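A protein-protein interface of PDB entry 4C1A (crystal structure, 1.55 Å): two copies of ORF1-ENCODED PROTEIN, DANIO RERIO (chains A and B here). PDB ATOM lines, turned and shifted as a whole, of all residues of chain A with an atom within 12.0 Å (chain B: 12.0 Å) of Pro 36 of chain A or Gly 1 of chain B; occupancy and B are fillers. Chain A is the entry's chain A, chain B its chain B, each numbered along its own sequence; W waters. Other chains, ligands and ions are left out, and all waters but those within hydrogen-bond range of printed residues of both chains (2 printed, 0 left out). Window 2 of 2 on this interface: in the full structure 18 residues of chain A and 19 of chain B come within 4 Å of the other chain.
CD2 of Leu 28 of chain A touches CD2 of Leu 7 of chain B, 3.9 Å away.
CB of Glu 10 of chain B touches CD1 of Leu 28 of chain A, at 3.96 Å.
Arg 31 of chain A touches Leu 7 of chain B (C to CD1, 3.7 Å).
Met 4 of chain B touches Leu 32 of chain A.
Leu 32 of chain A touches Leu 7 of chain B.
Leu 32 of chain A touches Glu 8 of chain B.
CG1 of Val 35 of chain A touches CB of Ala 3 of chain B (3.99 Å).
Met 4 of chain B touches Val 35 of chain A.
Gly 1 of chain B touches Pro 36 of chain A.
Met 4 of chain B touches Pro 36 of chain A (CB to O, 3.99 Å).
Glu 30 of chain A touches none of the printed residues of chain B.
No residue of chain B comes within 4 Å of Ala 34 of chain A.
Printed residues of chain B within 4 Å of Pro 36 of chain A: Gly 1 and Met 4.
Gly 1 of chain B touches one residue of chain A.
No residue of chain A comes within 4 Å of Pro 2 of chain B.
Of the printed residues of chain A, Ala 3 of chain B touches Val 35.
No residue of chain A comes within 4 Å of Glu 5 of chain B.
Of the printed residues of chain A, Glu 8 of chain B touches Leu 32.
Leu 9 of chain B touches none of the printed residues of chain A.
Printed residues of chain A within 4 Å of Leu 11 of chain B: Leu 28, Arg 29 and Leu 32.
The nearest residue of chain A that does not touch Gly 1 of chain B is Val 35 of chain A (6.6 Å).
The nearest printed residue of chain B that does not touch Leu 28 of chain A is Ala 6 of chain B (6.2 Å).
Of the 11 printed residues of chain B, 7 touch a printed residue of chain A.
Hydrophobic or aromatic side chains of chain B within 4 Å of the printed part of chain A: Ala 3, Met 4, Leu 7 and Leu 11.
Hydrophobic or aromatic side chains of chain A that line the printed part of chain B: Leu 28, Leu 32 and Val 35.
Among the printed residues, 13 pairs touch across the chains.
No position is printed for both chains.
Water W2 lies within hydrogen-bond range of the backbone carbonyl oxygen of Pro 36 of chain A (2.7 Å), the backbone NH of Gly 1 of chain B (2.9 Å) and the backbone NH of Met 4 of chain B (3.0 Å).
Water W1 bridges the backbone NH of Gly 1 of chain B (3.1 Å) and the backbone carbonyl oxygen of Pro 36 of chain A (3.3 Å).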
ATOM      1  N   LEU A  28      12.571  19.141  -0.331  1.00  0.00           N
ATOM      2  CA  LEU A  28      12.344  20.344  -1.111  1.00  0.00           C
ATOM      3  C   LEU A  28      11.128  20.172  -2.020  1.00  0.00           C
ATOM      4  O   LEU A  28      10.325  21.104  -2.153  1.00  0.00           O
ATOM      5  CB  LEU A  28      13.548  20.693  -1.972  1.00  0.00           C
ATOM      6  CG  LEU A  28      14.760  21.236  -1.236  1.00  0.00           C
ATOM      7  CD1 LEU A  28      15.955  21.104  -2.129  1.00  0.00           C
ATOM      8  CD2 LEU A  28      14.603  22.699  -0.839  1.00  0.00           C
ATOM      9  N   ARG A  29      10.984  19.012  -2.649  1.00  0.00           N
ATOM     10  CA  ARG A  29       9.782  18.759  -3.445  1.00  0.00           C
ATOM     11  C   ARG A  29       8.537  18.859  -2.586  1.00  0.00           C
ATOM     12  O   ARG A  29       7.532  19.394  -3.043  1.00  0.00           O
ATOM     13  CB  ARG A  29       9.851  17.370  -4.116  1.00  0.00           C
ATOM     14  CG  ARG A  29      10.801  17.330  -5.282  1.00  0.00           C
ATOM     15  CD  ARG A  29      10.938  15.970  -5.903  1.00  0.00           C
ATOM     16  NE  ARG A  29      11.813  16.037  -7.063  1.00  0.00           N
ATOM     17  CZ  ARG A  29      12.459  15.001  -7.581  1.00  0.00           C
ATOM     18  NH1 ARG A  29      12.362  13.781  -7.049  1.00  0.00           N
ATOM     19  NH2 ARG A  29      13.223  15.169  -8.651  1.00  0.00           N
ATOM     20  N   GLU A  30       8.549  18.327  -1.366  1.00  0.00           N
ATOM     21  CA  GLU A  30       7.373  18.452  -0.508  1.00  0.00           C
ATOM     22  C   GLU A  30       7.025  19.925  -0.257  1.00  0.00           C
ATOM     23  O   GLU A  30       5.862  20.347  -0.256  1.00  0.00           O
ATOM     24  CB  GLU A  30       7.596  17.716   0.826  1.00  0.00           C
ATOM     25  CG  GLU A  30       7.353  16.216   0.750  1.00  0.00           C
ATOM     26  CD  GLU A  30       7.797  15.454   2.011  1.00  0.00           C
ATOM     27  OE1 GLU A  30       8.849  15.804   2.605  1.00  0.00           O
ATOM     28  OE2 GLU A  30       7.085  14.498   2.399  1.00  0.00           O
ATOM     29  N   ARG A  31       8.044  20.708  -0.027  1.00  0.00           N
ATOM     30  CA  ARG A  31       7.840  22.107   0.255  1.00  0.00           C
ATOM     31  C   ARG A  31       7.314  22.846  -0.936  1.00  0.00           C
ATOM     32  O   ARG A  31       6.499  23.788  -0.804  1.00  0.00           O
ATOM     33  CB  ARG A  31       9.156  22.734   0.698  1.00  0.00           C
ATOM     34  CG  ARG A  31       9.548  22.499   2.133  1.00  0.00           C
ATOM     35  CD  ARG A  31       8.497  22.857   3.152  1.00  0.00           C
ATOM     36  NE  ARG A  31       9.032  22.817   4.511  1.00  0.00           N
ATOM     37  CZ  ARG A  31       8.893  21.804   5.358  1.00  0.00           C
ATOM     38  NH1 ARG A  31       8.232  20.707   5.007  1.00  0.00           N
ATOM     39  NH2 ARG A  31       9.417  21.894   6.576  1.00  0.00           N
ATOM     40  N   LEU A  32       7.813  22.465  -2.101  1.00  0.00           N
ATOM     41  CA  LEU A  32       7.414  23.115  -3.337  1.00  0.00           C
ATOM     42  C   LEU A  32       5.907  22.964  -3.484  1.00  0.00           C
ATOM     43  O   LEU A  32       5.206  23.869  -3.946  1.00  0.00           O
ATOM     44  CB  LEU A  32       8.173  22.493  -4.515  1.00  0.00           C
ATOM     45  CG  LEU A  32       7.822  22.855  -5.948  1.00  0.00           C
ATOM     46  CD1 LEU A  32       8.304  24.253  -6.237  1.00  0.00           C
ATOM     47  CD2 LEU A  32       8.437  21.849  -6.929  1.00  0.00           C
ATOM     48  N   LEU A  33       5.383  21.834  -3.050  1.00  0.00           N
ATOM     49  CA  LEU A  33       3.961  21.583  -3.169  1.00  0.00           C
ATOM     50  C   LEU A  33       3.133  22.304  -2.078  1.00  0.00           C
ATOM     51  O   LEU A  33       1.896  22.257  -2.088  1.00  0.00           O
ATOM     52  CB  LEU A  33       3.725  20.073  -3.150  1.00  0.00           C
ATOM     53  CG  LEU A  33       4.492  19.338  -4.253  1.00  0.00           C
ATOM     54  CD1 LEU A  33       4.359  17.850  -4.073  1.00  0.00           C
ATOM     55  CD2 LEU A  33       4.032  19.712  -5.636  1.00  0.00           C
ATOM     56  N   ALA A  34       3.818  22.989  -1.167  1.00  0.00           N
ATOM     57  CA  ALA A  34       3.194  23.636   0.005  1.00  0.00           C
ATOM     58  C   ALA A  34       3.163  25.156  -0.063  1.00  0.00           C
ATOM     59  O   ALA A  34       2.748  25.821   0.894  1.00  0.00           O
ATOM     60  CB  ALA A  34       3.917  23.214   1.277  1.00  0.00           C
ATOM     61  N   VAL A  35       3.625  25.713  -1.170  1.00  0.00           N
ATOM     62  CA  VAL A  35       3.607  27.160  -1.328  1.00  0.00           C
ATOM     63  C   VAL A  35       2.697  27.492  -2.505  1.00  0.00           C
ATOM     64  O   VAL A  35       2.350  26.601  -3.290  1.00  0.00           O
ATOM     65  CB  VAL A  35       5.039  27.742  -1.520  1.00  0.00           C
ATOM     66  CG1 VAL A  35       5.875  27.470  -0.301  1.00  0.00           C
ATOM     67  CG2 VAL A  35       5.729  27.181  -2.745  1.00  0.00           C
ATOM     68  N   PRO A  36       2.272  28.762  -2.622  1.00  0.00           N
ATOM     69  CA  PRO A  36       1.479  29.132  -3.799  1.00  0.00           C
ATOM     70  C   PRO A  36       2.229  28.916  -5.110  1.00  0.00           C
ATOM     71  O   PRO A  36       3.382  29.343  -5.219  1.00  0.00           O
ATOM     72  CB  PRO A  36       1.218  30.614  -3.587  1.00  0.00           C
ATOM     73  CG  PRO A  36       1.265  30.784  -2.078  1.00  0.00           C
ATOM     74  CD  PRO A  36       2.313  29.825  -1.603  1.00  0.00           C
ATOM     75  N   GLY B   1       5.191  32.117  -7.223  1.00  0.00           N
ATOM     76  CA  GLY B   1       5.723  33.340  -6.637  1.00  0.00           C
ATOM     77  C   GLY B   1       7.164  33.113  -6.201  1.00  0.00           C
ATOM     78  O   GLY B   1       7.760  32.120  -6.599  1.00  0.00           O
ATOM     79  N   PRO B   2       7.728  34.033  -5.409  1.00  0.00           N
ATOM     80  CA  PRO B   2       9.119  33.970  -4.960  1.00  0.00           C
ATOM     81  C   PRO B   2       9.469  32.698  -4.170  1.00  0.00           C
ATOM     82  O   PRO B   2      10.615  32.219  -4.252  1.00  0.00           O
ATOM     83  CB  PRO B   2       9.270  35.209  -4.065  1.00  0.00           C
ATOM     84  CG  PRO B   2       7.936  35.648  -3.771  1.00  0.00           C
ATOM     85  CD  PRO B   2       7.062  35.242  -4.895  1.00  0.00           C
ATOM     86  N   ALA B   3       8.546  32.174  -3.383  1.00  0.00           N
ATOM     87  CA  ALA B   3       8.898  30.982  -2.615  1.00  0.00           C
ATOM     88  C   ALA B   3       9.077  29.791  -3.531  1.00  0.00           C
ATOM     89  O   ALA B   3      10.008  28.989  -3.362  1.00  0.00           O
ATOM     90  CB  ALA B   3       7.858  30.692  -1.558  1.00  0.00           C
ATOM     91  N   MET B   4       8.201  29.668  -4.517  1.00  0.00           N
ATOM     92  CA  MET B   4       8.318  28.567  -5.471  1.00  0.00           C
ATOM     93  C   MET B   4       9.602  28.742  -6.268  1.00  0.00           C
ATOM     94  O   MET B   4      10.339  27.792  -6.465  1.00  0.00           O
ATOM     95  CB  MET B   4       7.099  28.529  -6.406  1.00  0.00           C
ATOM     96  CG  MET B   4       7.155  27.408  -7.432  1.00  0.00           C
ATOM     97  SD  MET B   4       5.832  27.428  -8.670  1.00  0.00           S
ATOM     98  CE  MET B   4       6.394  28.713  -9.793  1.00  0.00           C
ATOM     99  N   GLU B   5       9.923  29.973  -6.665  1.00  0.00           N
ATOM    100  CA  GLU B   5      11.129  30.201  -7.444  1.00  0.00           C
ATOM    101  C   GLU B   5      12.402  29.819  -6.690  1.00  0.00           C
ATOM    102  O   GLU B   5      13.341  29.209  -7.239  1.00  0.00           O
ATOM    103  CB  GLU B   5      11.187  31.647  -7.907  1.00  0.00           C
ATOM    104  CG  GLU B   5      10.025  32.031  -8.782  1.00  0.00           C
ATOM    105  CD  GLU B   5       9.886  33.523  -8.928  1.00  0.00           C
ATOM    106  OE1 GLU B   5      10.818  34.239  -8.518  1.00  0.00           O
ATOM    107  OE2 GLU B   5       8.847  33.969  -9.460  1.00  0.00           O
ATOM    108  N   ALA B   6      12.412  30.103  -5.400  1.00  0.00           N
ATOM    109  CA  ALA B   6      13.533  29.764  -4.552  1.00  0.00           C
ATOM    110  C   ALA B   6      13.695  28.254  -4.410  1.00  0.00           C
ATOM    111  O   ALA B   6      14.815  27.740  -4.511  1.00  0.00           O
ATOM    112  CB  ALA B   6      13.382  30.430  -3.181  1.00  0.00           C
ATOM    113  N   LEU B   7      12.604  27.552  -4.139  1.00  0.00           N
ATOM    114  CA  LEU B   7      12.651  26.108  -4.005  1.00  0.00           C
ATOM    115  C   LEU B   7      13.055  25.422  -5.315  1.00  0.00           C
ATOM    116  O   LEU B   7      13.797  24.428  -5.317  1.00  0.00           O
ATOM    117  CB  LEU B   7      11.294  25.627  -3.513  1.00  0.00           C
ATOM    118  CG  LEU B   7      10.979  26.025  -2.062  1.00  0.00           C
ATOM    119  CD1 LEU B   7       9.553  25.667  -1.729  1.00  0.00           C
ATOM    120  CD2 LEU B   7      11.874  25.414  -1.013  1.00  0.00           C
ATOM    121  N   GLU B   8      12.613  25.974  -6.434  1.00  0.00           N
ATOM    122  CA  GLU B   8      12.950  25.393  -7.725  1.00  0.00           C
ATOM    123  C   GLU B   8      14.448  25.519  -7.978  1.00  0.00           C
ATOM    124  O   GLU B   8      15.057  24.598  -8.511  1.00  0.00           O
ATOM    125  CB  GLU B   8      12.157  26.055  -8.852  1.00  0.00           C
ATOM    126  CG  GLU B   8      10.690  25.728  -8.849  1.00  0.00           C
ATOM    127  CD  GLU B   8       9.858  26.593  -9.821  1.00  0.00           C
ATOM    128  OE1 GLU B   8      10.379  27.580 -10.380  1.00  0.00           O
ATOM    129  OE2 GLU B   8       8.664  26.287 -10.008  1.00  0.00           O
ATOM    130  N   LEU B   9      15.041  26.656  -7.599  1.00  0.00           N
ATOM    131  CA  LEU B   9      16.493  26.830  -7.700  1.00  0.00           C
ATOM    132  C   LEU B   9      17.259  25.840  -6.848  1.00  0.00           C
ATOM    133  O   LEU B   9      18.221  25.224  -7.324  1.00  0.00           O
ATOM    134  CB  LEU B   9      16.892  28.280  -7.309  1.00  0.00           C
ATOM    135  CG  LEU B   9      18.384  28.666  -7.418  1.00  0.00           C
ATOM    136  CD1 LEU B   9      18.872  28.502  -8.847  1.00  0.00           C
ATOM    137  CD2 LEU B   9      18.616  30.078  -6.907  1.00  0.00           C
ATOM    138  N   GLU B  10      16.842  25.670  -5.599  1.00  0.00           N
ATOM    139  CA  GLU B  10      17.501  24.715  -4.715  1.00  0.00           C
ATOM    140  C   GLU B  10      17.380  23.328  -5.285  1.00  0.00           C
ATOM    141  O   GLU B  10      18.326  22.538  -5.197  1.00  0.00           O
ATOM    142  CB  GLU B  10      16.939  24.755  -3.293  1.00  0.00           C
ATOM    143  CG  GLU B  10      17.170  26.112  -2.552  1.00  0.00           C
ATOM    144  CD  GLU B  10      18.624  26.500  -2.459  1.00  0.00           C
ATOM    145  OE1 GLU B  10      19.372  25.877  -1.668  1.00  0.00           O
ATOM    146  OE2 GLU B  10      19.049  27.460  -3.171  1.00  0.00           O
ATOM    147  N   LEU B  11      16.211  23.006  -5.851  1.00  0.00           N
ATOM    148  CA  LEU B  11      16.022  21.688  -6.486  1.00  0.00           C
ATOM    149  C   LEU B  11      16.955  21.484  -7.695  1.00  0.00           C
ATOM    150  O   LEU B  11      17.515  20.402  -7.886  1.00  0.00           O
ATOM    151  CB  LEU B  11      14.562  21.503  -6.886  1.00  0.00           C
ATOM    152  CG  LEU B  11      13.691  20.998  -5.750  1.00  0.00           C
ATOM    153  CD1 LEU B  11      12.257  21.222  -6.091  1.00  0.00           C
ATOM    154  CD2 LEU B  11      13.952  19.539  -5.536  1.00  0.00           C
HETATM  155  O   HOH W   1       2.112  31.823  -7.068  1.00  0.00           O
HETATM  156  O   HOH W   2       5.480  30.936  -4.591  1.00  0.00           O
